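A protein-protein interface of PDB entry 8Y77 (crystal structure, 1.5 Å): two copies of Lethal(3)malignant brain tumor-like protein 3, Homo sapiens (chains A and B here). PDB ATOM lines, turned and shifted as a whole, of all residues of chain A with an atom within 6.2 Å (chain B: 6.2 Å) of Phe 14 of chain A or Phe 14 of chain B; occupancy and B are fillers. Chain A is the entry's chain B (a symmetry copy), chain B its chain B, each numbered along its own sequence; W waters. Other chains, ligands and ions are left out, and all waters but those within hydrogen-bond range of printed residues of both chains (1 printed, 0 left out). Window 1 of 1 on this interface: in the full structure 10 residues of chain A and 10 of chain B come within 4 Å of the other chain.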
ATOM      1  N   TRP A   6      -4.894   4.974 -37.485  1.00  0.00           N
ATOM      2  CA  TRP A   6      -6.172   4.346 -37.166  1.00  0.00           C
ATOM      3  C   TRP A   6      -6.690   3.525 -38.340  1.00  0.00           C
ATOM      4  O   TRP A   6      -6.538   3.904 -39.504  1.00  0.00           O
ATOM      5  CB  TRP A   6      -7.216   5.416 -36.858  1.00  0.00           C
ATOM      6  CG  TRP A   6      -7.173   5.991 -35.477  1.00  0.00           C
ATOM      7  CD1 TRP A   6      -6.178   5.859 -34.553  1.00  0.00           C
ATOM      8  CD2 TRP A   6      -8.184   6.802 -34.869  1.00  0.00           C
ATOM      9  NE1 TRP A   6      -6.508   6.544 -33.406  1.00  0.00           N
ATOM     10  CE2 TRP A   6      -7.739   7.123 -33.574  1.00  0.00           C
ATOM     11  CE3 TRP A   6      -9.426   7.277 -35.296  1.00  0.00           C
ATOM     12  CZ2 TRP A   6      -8.487   7.917 -32.704  1.00  0.00           C
ATOM     13  CZ3 TRP A   6     -10.173   8.065 -34.433  1.00  0.00           C
ATOM     14  CH2 TRP A   6      -9.699   8.374 -33.150  1.00  0.00           C
ATOM     15  N   ASP A   9     -12.140   0.787 -39.202  1.00  0.00           N
ATOM     16  CA  ASP A   9     -13.116   0.536 -38.144  1.00  0.00           C
ATOM     17  C   ASP A   9     -12.997   1.562 -37.028  1.00  0.00           C
ATOM     18  O   ASP A   9     -14.010   1.995 -36.468  1.00  0.00           O
ATOM     19  CB  ASP A   9     -12.957  -0.876 -37.587  1.00  0.00           C
ATOM     20  CG  ASP A   9     -14.224  -1.376 -36.896  1.00  0.00           C
ATOM     21  OD1 ASP A   9     -14.130  -1.900 -35.765  1.00  0.00           O
ATOM     22  OD2 ASP A   9     -15.322  -1.248 -37.482  1.00  0.00           O
ATOM     23  N   GLU A  10     -11.771   1.959 -36.680  1.00  0.00           N
ATOM     24  CA  GLU A  10     -11.592   2.962 -35.634  1.00  0.00           C
ATOM     25  C   GLU A  10     -12.212   4.294 -36.024  1.00  0.00           C
ATOM     26  O   GLU A  10     -12.801   4.979 -35.182  1.00  0.00           O
ATOM     27  CB  GLU A  10     -10.108   3.161 -35.350  1.00  0.00           C
ATOM     28  CG  GLU A  10      -9.535   2.180 -34.373  1.00  0.00           C
ATOM     29  CD  GLU A  10      -8.073   2.466 -34.117  1.00  0.00           C
ATOM     30  OE1 GLU A  10      -7.226   2.006 -34.914  1.00  0.00           O
ATOM     31  OE2 GLU A  10      -7.772   3.178 -33.141  1.00  0.00           O
ATOM     32  N   VAL A  11     -12.056   4.699 -37.286  1.00  0.00           N
ATOM     33  CA  VAL A  11     -12.653   5.956 -37.732  1.00  0.00           C
ATOM     34  C   VAL A  11     -14.170   5.873 -37.623  1.00  0.00           C
ATOM     35  O   VAL A  11     -14.830   6.785 -37.102  1.00  0.00           O
ATOM     36  CB  VAL A  11     -12.202   6.274 -39.169  1.00  0.00           C
ATOM     37  CG1 VAL A  11     -12.987   7.465 -39.732  1.00  0.00           C
ATOM     38  CG2 VAL A  11     -10.699   6.569 -39.199  1.00  0.00           C
ATOM     39  N   SER A  12     -14.738   4.763 -38.096  1.00  0.00           N
ATOM     40  CA  SER A  12     -16.186   4.589 -38.070  1.00  0.00           C
ATOM     41  C   SER A  12     -16.708   4.605 -36.639  1.00  0.00           C
ATOM     42  O   SER A  12     -17.720   5.249 -36.339  1.00  0.00           O
ATOM     43  CB  SER A  12     -16.550   3.265 -38.738  1.00  0.00           C
ATOM     44  OG  SER A  12     -17.910   2.951 -38.465  1.00  0.00           O
ATOM     45  N   GLU A  13     -16.026   3.892 -35.742  1.00  0.00           N
ATOM     46  CA  GLU A  13     -16.469   3.841 -34.355  1.00  0.00           C
ATOM     47  C   GLU A  13     -16.347   5.204 -33.686  1.00  0.00           C
ATOM     48  O   GLU A  13     -17.211   5.589 -32.883  1.00  0.00           O
ATOM     49  CB  GLU A  13     -15.661   2.796 -33.595  1.00  0.00           C
ATOM     50  CG  GLU A  13     -15.952   1.356 -34.025  1.00  0.00           C
ATOM     51  CD  GLU A  13     -17.299   0.858 -33.543  1.00  0.00           C
ATOM     52  OE1 GLU A  13     -18.157   0.517 -34.392  1.00  0.00           O
ATOM     53  OE2 GLU A  13     -17.491   0.800 -32.312  1.00  0.00           O
ATOM     54  N   PHE A  14     -15.292   5.962 -34.008  1.00  0.00           N
ATOM     55  CA  PHE A  14     -15.191   7.316 -33.472  1.00  0.00           C
ATOM     56  C   PHE A  14     -16.360   8.181 -33.927  1.00  0.00           C
ATOM     57  O   PHE A  14     -16.980   8.884 -33.120  1.00  0.00           O
ATOM     58  CB  PHE A  14     -13.870   7.992 -33.858  1.00  0.00           C
ATOM     59  CG  PHE A  14     -13.756   9.373 -33.280  1.00  0.00           C
ATOM     60  CD1 PHE A  14     -13.350   9.538 -31.971  1.00  0.00           C
ATOM     61  CD2 PHE A  14     -14.137  10.491 -34.013  1.00  0.00           C
ATOM     62  CE1 PHE A  14     -13.287  10.794 -31.396  1.00  0.00           C
ATOM     63  CE2 PHE A  14     -14.076  11.754 -33.445  1.00  0.00           C
ATOM     64  CZ  PHE A  14     -13.648  11.902 -32.134  1.00  0.00           C
ATOM     65  N   ILE A  15     -16.666   8.155 -35.227  1.00  0.00           N
ATOM     66  CA  ILE A  15     -17.763   8.969 -35.738  1.00  0.00           C
ATOM     67  C   ILE A  15     -19.071   8.610 -35.042  1.00  0.00           C
ATOM     68  O   ILE A  15     -19.842   9.493 -34.646  1.00  0.00           O
ATOM     69  CB  ILE A  15     -17.835   8.854 -37.273  1.00  0.00           C
ATOM     70  CG1 ILE A  15     -16.637   9.570 -37.903  1.00  0.00           C
ATOM     71  CG2 ILE A  15     -19.164   9.411 -37.801  1.00  0.00           C
ATOM     72  CD1 ILE A  15     -16.405   9.189 -39.349  1.00  0.00           C
ATOM     73  N   GLN A  16     -19.312   7.312 -34.828  1.00  0.00           N
ATOM     74  CA  GLN A  16     -20.545   6.879 -34.181  1.00  0.00           C
ATOM     75  C   GLN A  16     -20.654   7.363 -32.749  1.00  0.00           C
ATOM     76  O   GLN A  16     -21.769   7.429 -32.218  1.00  0.00           O
ATOM     77  CB  GLN A  16     -20.632   5.356 -34.179  1.00  0.00           C
ATOM     78  CG  GLN A  16     -20.841   4.753 -35.554  1.00  0.00           C
ATOM     79  CD  GLN A  16     -20.793   3.240 -35.508  1.00  0.00           C
ATOM     80  OE1 GLN A  16     -21.638   2.612 -34.880  1.00  0.00           O
ATOM     81  NE2 GLN A  16     -19.801   2.648 -36.166  1.00  0.00           N
ATOM     82  N   SER A  17     -19.531   7.693 -32.109  1.00  0.00           N
ATOM     83  CA  SER A  17     -19.581   8.198 -30.741  1.00  0.00           C
ATOM     84  C   SER A  17     -19.918   9.682 -30.659  1.00  0.00           C
ATOM     85  O   SER A  17     -20.174  10.184 -29.553  1.00  0.00           O
ATOM     86  CB  SER A  17     -18.273   7.895 -30.002  1.00  0.00           C
ATOM     87  OG  SER A  17     -17.232   8.768 -30.417  1.00  0.00           O
ATOM     88  N   LEU A  18     -19.930  10.400 -31.783  1.00  0.00           N
ATOM     89  CA  LEU A  18     -20.302  11.807 -31.787  1.00  0.00           C
ATOM     90  C   LEU A  18     -21.823  11.928 -31.761  1.00  0.00           C
ATOM     91  O   LEU A  18     -22.521  11.125 -32.389  1.00  0.00           O
ATOM     92  CB  LEU A  18     -19.754  12.516 -33.031  1.00  0.00           C
ATOM     93  CG  LEU A  18     -18.231  12.494 -33.207  1.00  0.00           C
ATOM     94  CD1 LEU A  18     -17.844  13.131 -34.539  1.00  0.00           C
ATOM     95  CD2 LEU A  18     -17.514  13.180 -32.047  1.00  0.00           C
ATOM     96  N   PHE A  38      -9.087   9.866 -43.559  1.00  0.00           N
ATOM     97  CA  PHE A  38      -9.920  10.767 -42.762  1.00  0.00           C
ATOM     98  C   PHE A  38      -9.301  12.155 -42.670  1.00  0.00           C
ATOM     99  O   PHE A  38     -10.000  13.166 -42.793  1.00  0.00           O
ATOM    100  CB  PHE A  38     -10.071  10.161 -41.359  1.00  0.00           C
ATOM    101  CG  PHE A  38     -11.175  10.758 -40.508  1.00  0.00           C
ATOM    102  CD1 PHE A  38     -12.420  11.062 -41.037  1.00  0.00           C
ATOM    103  CD2 PHE A  38     -10.964  10.943 -39.155  1.00  0.00           C
ATOM    104  CE1 PHE A  38     -13.422  11.562 -40.224  1.00  0.00           C
ATOM    105  CE2 PHE A  38     -11.960  11.451 -38.336  1.00  0.00           C
ATOM    106  CZ  PHE A  38     -13.190  11.752 -38.874  1.00  0.00           C
ATOM    107  N   LYS A  59     -19.633  18.466 -36.921  1.00  0.00           N
ATOM    108  CA  LYS A  59     -19.032  17.762 -35.791  1.00  0.00           C
ATOM    109  C   LYS A  59     -17.897  16.858 -36.259  1.00  0.00           C
ATOM    110  O   LYS A  59     -16.842  16.784 -35.613  1.00  0.00           O
ATOM    111  CB  LYS A  59     -20.097  16.956 -35.043  1.00  0.00           C
ATOM    112  CG  LYS A  59     -21.195  17.801 -34.401  1.00  0.00           C
ATOM    113  CD  LYS A  59     -22.268  16.920 -33.789  1.00  0.00           C
ATOM    114  CE  LYS A  59     -23.463  17.743 -33.320  1.00  0.00           C
ATOM    115  NZ  LYS A  59     -24.552  16.845 -32.847  1.00  0.00           N
ATOM    116  N   ILE A  60     -18.090  16.171 -37.384  1.00  0.00           N
ATOM    117  CA  ILE A  60     -17.035  15.317 -37.917  1.00  0.00           C
ATOM    118  C   ILE A  60     -15.830  16.148 -38.353  1.00  0.00           C
ATOM    119  O   ILE A  60     -14.679  15.808 -38.046  1.00  0.00           O
ATOM    120  CB  ILE A  60     -17.583  14.443 -39.058  1.00  0.00           C
ATOM    121  CG1 ILE A  60     -18.707  13.541 -38.536  1.00  0.00           C
ATOM    122  CG2 ILE A  60     -16.468  13.594 -39.666  1.00  0.00           C
ATOM    123  CD1 ILE A  60     -19.511  12.878 -39.646  1.00  0.00           C
ATOM    124  N   SER A  63     -13.758  17.370 -35.572  1.00  0.00           N
ATOM    125  CA  SER A  63     -12.874  16.316 -35.085  1.00  0.00           C
ATOM    126  C   SER A  63     -11.662  16.165 -35.990  1.00  0.00           C
ATOM    127  O   SER A  63     -10.533  16.028 -35.506  1.00  0.00           O
ATOM    128  CB  SER A  63     -13.635  14.998 -34.969  1.00  0.00           C
ATOM    129  OG  SER A  63     -14.767  15.144 -34.117  1.00  0.00           O
ATOM    130  N   PHE A  67      -7.749  16.383 -34.929  1.00  0.00           N
ATOM    131  CA  PHE A  67      -6.827  15.284 -35.205  1.00  0.00           C
ATOM    132  C   PHE A  67      -5.650  15.755 -36.052  1.00  0.00           C
ATOM    133  O   PHE A  67      -4.506  15.347 -35.823  1.00  0.00           O
ATOM    134  CB  PHE A  67      -7.563  14.151 -35.927  1.00  0.00           C
ATOM    135  CG  PHE A  67      -8.621  13.448 -35.092  1.00  0.00           C
ATOM    136  CD1 PHE A  67      -8.645  13.555 -33.718  1.00  0.00           C
ATOM    137  CD2 PHE A  67      -9.592  12.682 -35.716  1.00  0.00           C
ATOM    138  CE1 PHE A  67      -9.622  12.901 -32.976  1.00  0.00           C
ATOM    139  CE2 PHE A  67     -10.571  12.026 -34.982  1.00  0.00           C
ATOM    140  CZ  PHE A  67     -10.580  12.135 -33.612  1.00  0.00           C
ATOM    141  N   TRP B   6     -24.654   7.794 -21.151  1.00  0.00           N
ATOM    142  CA  TRP B   6     -23.415   7.033 -21.278  1.00  0.00           C
ATOM    143  C   TRP B   6     -22.936   6.532 -19.922  1.00  0.00           C
ATOM    144  O   TRP B   6     -23.057   7.220 -18.905  1.00  0.00           O
ATOM    145  CB  TRP B   6     -22.315   7.918 -21.857  1.00  0.00           C
ATOM    146  CG  TRP B   6     -22.337   8.100 -23.342  1.00  0.00           C
ATOM    147  CD1 TRP B   6     -23.345   7.778 -24.203  1.00  0.00           C
ATOM    148  CD2 TRP B   6     -21.287   8.658 -24.139  1.00  0.00           C
ATOM    149  NE1 TRP B   6     -22.986   8.107 -25.490  1.00  0.00           N
ATOM    150  CE2 TRP B   6     -21.723   8.641 -25.476  1.00  0.00           C
ATOM    151  CE3 TRP B   6     -20.017   9.160 -23.846  1.00  0.00           C
ATOM    152  CZ2 TRP B   6     -20.939   9.126 -26.523  1.00  0.00           C
ATOM    153  CZ3 TRP B   6     -19.234   9.642 -24.885  1.00  0.00           C
ATOM    154  CH2 TRP B   6     -19.699   9.618 -26.208  1.00  0.00           C
ATOM    155  N   ASP B   9     -17.640   3.829 -18.309  1.00  0.00           N
ATOM    156  CA  ASP B   9     -16.688   3.246 -19.252  1.00  0.00           C
ATOM    157  C   ASP B   9     -16.758   3.937 -20.605  1.00  0.00           C
ATOM    158  O   ASP B   9     -15.727   4.144 -21.253  1.00  0.00           O
ATOM    159  CB  ASP B   9     -16.931   1.747 -19.406  1.00  0.00           C
ATOM    160  CG  ASP B   9     -15.699   1.009 -19.927  1.00  0.00           C
ATOM    161  OD1 ASP B   9     -15.831   0.204 -20.874  1.00  0.00           O
ATOM    162  OD2 ASP B   9     -14.592   1.230 -19.389  1.00  0.00           O
ATOM    163  N   GLU B  10     -17.963   4.293 -21.057  1.00  0.00           N
ATOM    164  CA  GLU B  10     -18.094   4.983 -22.337  1.00  0.00           C
ATOM    165  C   GLU B  10     -17.397   6.335 -22.317  1.00  0.00           C
ATOM    166  O   GLU B  10     -16.777   6.732 -23.308  1.00  0.00           O
ATOM    167  CB  GLU B  10     -19.566   5.181 -22.675  1.00  0.00           C
ATOM    168  CG  GLU B  10     -20.201   4.006 -23.355  1.00  0.00           C
ATOM    169  CD  GLU B  10     -21.646   4.293 -23.690  1.00  0.00           C
ATOM    170  OE1 GLU B  10     -22.512   4.115 -22.805  1.00  0.00           O
ATOM    171  OE2 GLU B  10     -21.915   4.730 -24.824  1.00  0.00           O
ATOM    172  N   VAL B  11     -17.520   7.074 -21.213  1.00  0.00           N
ATOM    173  CA  VAL B  11     -16.850   8.370 -21.119  1.00  0.00           C
ATOM    174  C   VAL B  11     -15.341   8.176 -21.190  1.00  0.00           C
ATOM    175  O   VAL B  11     -14.636   8.874 -21.933  1.00  0.00           O
ATOM    176  CB  VAL B  11     -17.272   9.090 -19.826  1.00  0.00           C
ATOM    177  CG1 VAL B  11     -16.417  10.342 -19.600  1.00  0.00           C
ATOM    178  CG2 VAL B  11     -18.755   9.466 -19.888  1.00  0.00           C
ATOM    179  N   SER B  12     -14.833   7.205 -20.429  1.00  0.00           N
ATOM    180  CA  SER B  12     -13.397   6.949 -20.396  1.00  0.00           C
ATOM    181  C   SER B  12     -12.886   6.548 -21.774  1.00  0.00           C
ATOM    182  O   SER B  12     -11.842   7.029 -22.230  1.00  0.00           O
ATOM    183  CB  SER B  12     -13.102   5.837 -19.392  1.00  0.00           C
ATOM    184  OG  SER B  12     -11.764   5.386 -19.560  1.00  0.00           O
ATOM    185  N   GLU B  13     -13.614   5.659 -22.450  1.00  0.00           N
ATOM    186  CA  GLU B  13     -13.185   5.209 -23.768  1.00  0.00           C
ATOM    187  C   GLU B  13     -13.236   6.345 -24.782  1.00  0.00           C
ATOM    188  O   GLU B  13     -12.357   6.448 -25.652  1.00  0.00           O
ATOM    189  CB  GLU B  13     -14.057   4.044 -24.223  1.00  0.00           C
ATOM    190  CG  GLU B  13     -13.843   2.761 -23.416  1.00  0.00           C
ATOM    191  CD  GLU B  13     -12.530   2.076 -23.735  1.00  0.00           C
ATOM    192  OE1 GLU B  13     -11.686   1.930 -22.819  1.00  0.00           O
ATOM    193  OE2 GLU B  13     -12.351   1.676 -24.903  1.00  0.00           O
ATOM    194  N   PHE B  14     -14.244   7.219 -24.685  1.00  0.00           N
ATOM    195  CA  PHE B  14     -14.273   8.381 -25.568  1.00  0.00           C
ATOM    196  C   PHE B  14     -13.054   9.270 -25.355  1.00  0.00           C
ATOM    197  O   PHE B  14     -12.402   9.692 -26.318  1.00  0.00           O
ATOM    198  CB  PHE B  14     -15.552   9.209 -25.390  1.00  0.00           C
ATOM    199  CG  PHE B  14     -15.592  10.386 -26.321  1.00  0.00           C
ATOM    200  CD1 PHE B  14     -15.998  10.213 -27.629  1.00  0.00           C
ATOM    201  CD2 PHE B  14     -15.144  11.638 -25.915  1.00  0.00           C
ATOM    202  CE1 PHE B  14     -15.995  11.268 -28.523  1.00  0.00           C
ATOM    203  CE2 PHE B  14     -15.138  12.702 -26.804  1.00  0.00           C
ATOM    204  CZ  PHE B  14     -15.567  12.512 -28.110  1.00  0.00           C
ATOM    205  N   ILE B  15     -12.740   9.580 -24.095  1.00  0.00           N
ATOM    206  CA  ILE B  15     -11.596  10.439 -23.815  1.00  0.00           C
ATOM    207  C   ILE B  15     -10.315   9.832 -24.378  1.00  0.00           C
ATOM    208  O   ILE B  15      -9.499  10.530 -24.992  1.00  0.00           O
ATOM    209  CB  ILE B  15     -11.517  10.740 -22.306  1.00  0.00           C
ATOM    210  CG1 ILE B  15     -12.669  11.666 -21.902  1.00  0.00           C
ATOM    211  CG2 ILE B  15     -10.155  11.344 -21.938  1.00  0.00           C
ATOM    212  CD1 ILE B  15     -12.911  11.704 -20.409  1.00  0.00           C
ATOM    213  N   GLN B  16     -10.148   8.513 -24.230  1.00  0.00           N
ATOM    214  CA  GLN B  16      -8.947   7.853 -24.726  1.00  0.00           C
ATOM    215  C   GLN B  16      -8.822   7.924 -26.235  1.00  0.00           C
ATOM    216  O   GLN B  16      -7.709   7.782 -26.755  1.00  0.00           O
ATOM    217  CB  GLN B  16      -8.945   6.384 -24.316  1.00  0.00           C
ATOM    218  CG  GLN B  16      -8.759   6.165 -22.827  1.00  0.00           C
ATOM    219  CD  GLN B  16      -8.893   4.701 -22.462  1.00  0.00           C
ATOM    220  OE1 GLN B  16      -8.089   3.880 -22.889  1.00  0.00           O
ATOM    221  NE2 GLN B  16      -9.911   4.366 -21.676  1.00  0.00           N
ATOM    222  N   SER B  17      -9.930   8.131 -26.949  1.00  0.00           N
ATOM    223  CA  SER B  17      -9.862   8.243 -28.402  1.00  0.00           C
ATOM    224  C   SER B  17      -9.443   9.628 -28.881  1.00  0.00           C
ATOM    225  O   SER B  17      -9.168   9.797 -30.079  1.00  0.00           O
ATOM    226  CB  SER B  17     -11.190   7.825 -29.042  1.00  0.00           C
ATOM    227  OG  SER B  17     -12.178   8.835 -28.887  1.00  0.00           O
ATOM    228  N   LEU B  18      -9.382  10.622 -27.993  1.00  0.00           N
ATOM    229  CA  LEU B  18      -8.931  11.954 -28.367  1.00  0.00           C
ATOM    230  C   LEU B  18      -7.406  11.979 -28.413  1.00  0.00           C
ATOM    231  O   LEU B  18      -6.750  11.338 -27.586  1.00  0.00           O
ATOM    232  CB  LEU B  18      -9.430  13.003 -27.365  1.00  0.00           C
ATOM    233  CG  LEU B  18     -10.950  13.115 -27.202  1.00  0.00           C
ATOM    234  CD1 LEU B  18     -11.290  14.109 -26.095  1.00  0.00           C
ATOM    235  CD2 LEU B  18     -11.636  13.500 -28.510  1.00  0.00           C
ATOM    236  N   PHE B  38     -20.146  13.905 -16.596  1.00  0.00           N
ATOM    237  CA  PHE B  38     -19.270  14.508 -17.601  1.00  0.00           C
ATOM    238  C   PHE B  38     -19.812  15.852 -18.069  1.00  0.00           C
ATOM    239  O   PHE B  38     -19.056  16.817 -18.220  1.00  0.00           O
ATOM    240  CB  PHE B  38     -19.165  13.537 -18.786  1.00  0.00           C
ATOM    241  CG  PHE B  38     -18.036  13.819 -19.759  1.00  0.00           C
ATOM    242  CD1 PHE B  38     -16.771  14.184 -19.322  1.00  0.00           C
ATOM    243  CD2 PHE B  38     -18.247  13.642 -21.113  1.00  0.00           C
ATOM    244  CE1 PHE B  38     -15.749  14.389 -20.232  1.00  0.00           C
ATOM    245  CE2 PHE B  38     -17.230  13.853 -22.031  1.00  0.00           C
ATOM    246  CZ  PHE B  38     -15.980  14.219 -21.585  1.00  0.00           C
ATOM    247  N   LYS B  59      -9.187  19.781 -25.233  1.00  0.00           N
ATOM    248  CA  LYS B  59      -9.835  18.832 -26.134  1.00  0.00           C
ATOM    249  C   LYS B  59     -11.015  18.154 -25.448  1.00  0.00           C
ATOM    250  O   LYS B  59     -12.078  17.967 -26.058  1.00  0.00           O
ATOM    251  CB  LYS B  59      -8.823  17.796 -26.628  1.00  0.00           C
ATOM    252  CG  LYS B  59      -7.684  18.373 -27.466  1.00  0.00           C
ATOM    253  CD  LYS B  59      -6.667  17.300 -27.809  1.00  0.00           C
ATOM    254  CE  LYS B  59      -5.432  17.897 -28.474  1.00  0.00           C
ATOM    255  NZ  LYS B  59      -4.398  16.845 -28.678  1.00  0.00           N
ATOM    256  N   ILE B  60     -10.852  17.787 -24.178  1.00  0.00           N
ATOM    257  CA  ILE B  60     -11.950  17.170 -23.442  1.00  0.00           C
ATOM    258  C   ILE B  60     -13.102  18.154 -23.257  1.00  0.00           C
ATOM    259  O   ILE B  60     -14.273  17.809 -23.468  1.00  0.00           O
ATOM    260  CB  ILE B  60     -11.442  16.608 -22.102  1.00  0.00           C
ATOM    261  CG1 ILE B  60     -10.374  15.537 -22.352  1.00  0.00           C
ATOM    262  CG2 ILE B  60     -12.599  16.019 -21.296  1.00  0.00           C
ATOM    263  CD1 ILE B  60      -9.601  15.156 -21.098  1.00  0.00           C
ATOM    264  N   SER B  63     -15.125  18.691 -26.280  1.00  0.00           N
ATOM    265  CA  SER B  63     -16.070  17.597 -26.470  1.00  0.00           C
ATOM    266  C   SER B  63     -17.281  17.765 -25.568  1.00  0.00           C
ATOM    267  O   SER B  63     -18.420  17.565 -26.005  1.00  0.00           O
ATOM    268  CB  SER B  63     -15.385  16.256 -26.220  1.00  0.00           C
ATOM    269  OG  SER B  63     -14.253  16.103 -27.070  1.00  0.00           O
ATOM    270  N   PHE B  67     -21.184  17.906 -26.679  1.00  0.00           N
ATOM    271  CA  PHE B  67     -22.164  16.976 -26.122  1.00  0.00           C
ATOM    272  C   PHE B  67     -23.306  17.724 -25.443  1.00  0.00           C
ATOM    273  O   PHE B  67     -24.472  17.334 -25.562  1.00  0.00           O
ATOM    274  CB  PHE B  67     -21.487  16.042 -25.115  1.00  0.00           C
ATOM    275  CG  PHE B  67     -20.477  15.081 -25.720  1.00  0.00           C
ATOM    276  CD1 PHE B  67     -20.457  14.810 -27.072  1.00  0.00           C
ATOM    277  CD2 PHE B  67     -19.545  14.459 -24.905  1.00  0.00           C
ATOM    278  CE1 PHE B  67     -19.524  13.926 -27.601  1.00  0.00           C
ATOM    279  CE2 PHE B  67     -18.610  13.575 -25.426  1.00  0.00           C
ATOM    280  CZ  PHE B  67     -18.606  13.309 -26.774  1.00  0.00           C
HETATM  281  O   HOH W   1     -14.739   7.590 -29.485  1.00  0.00           O
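The side-chain hydroxyl of Ser 17 of chain B is in hydrogen-bond range of the backbone carbonyl oxygen of Phe 14 of chain B. The backbone carbonyl oxygen (O) of Phe 14 of chain A lies within hydrogen-bond range of the side-chain hydroxyl (OG) of Ser 17 of chain A, 2.7 Å away.
Trp 6 of chain A touches Ser 17 of chain B. CE1 of Phe 14 of chain B touches CE1 of Phe 14 of chain A (3.98 Å). Phe 14 of chain A touches Ser 17 of chain B (CE1 to OG, 3.4 Å). CZ2 of Trp 6 of chain B touches O of Ser 17 of chain A (3.3 Å). CE1 of Phe 14 of chain B touches OG of Ser 17 of chain A (3.4 Å).
Phe 14 of chain A touches two residues of chain B. Phe 14 of chain B touches just these residues of chain A: Phe 14 and Ser 17. Of the printed residues of chain B, Ser 17 of chain A touches Trp 6 and Phe 14. Of the printed residues of chain B, Trp 6 of chain A touches Ser 17 (3.3 Å). Printed residues of chain A within 4 Å of Trp 6 of chain B: Ser 17 (3.3 Å). Of the printed residues of chain A, Ser 17 of chain B touches Trp 6 and Phe 14. The nearest residue of chain A that does not touch Phe 14 of chain B is Leu 18 of chain A (4.3 Å).
Printed residues of chain A that touch a printed residue of chain B: Trp 6, Phe 14 and Ser 17. Among the printed residues, no Asp or Glu carboxylate lies within 4 Å of a Lys or Arg side-chain nitrogen of the other chain.
Trp 6 of chain A touches Ser 17 of chain B, and with the chains exchanged Ser 17 of chain A touches Trp 6 of chain B. Phe 14 of chain A touches its own counterpart, Phe 14 of chain B. Phe 14 of chain A touches Ser 17 of chain B, and with the chains exchanged Ser 17 of chain A touches Phe 14 of chain B. Positions printed for both chains: 6, 9, 10, 11, 12, 13, 14, 15, 16, 17, 18, 38, 59, 60, 63 and 67. Of the 5 pairs that touch across the chains among the printed residues, 5 have their exchanged pair printed and touching as well.
Water W1 bridges the side-chain hydroxyl (OG) of Ser 17 of chain B (2.9 Å) and the side-chain hydroxyl (OG) of Ser 17 of chain A (2.9 Å).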
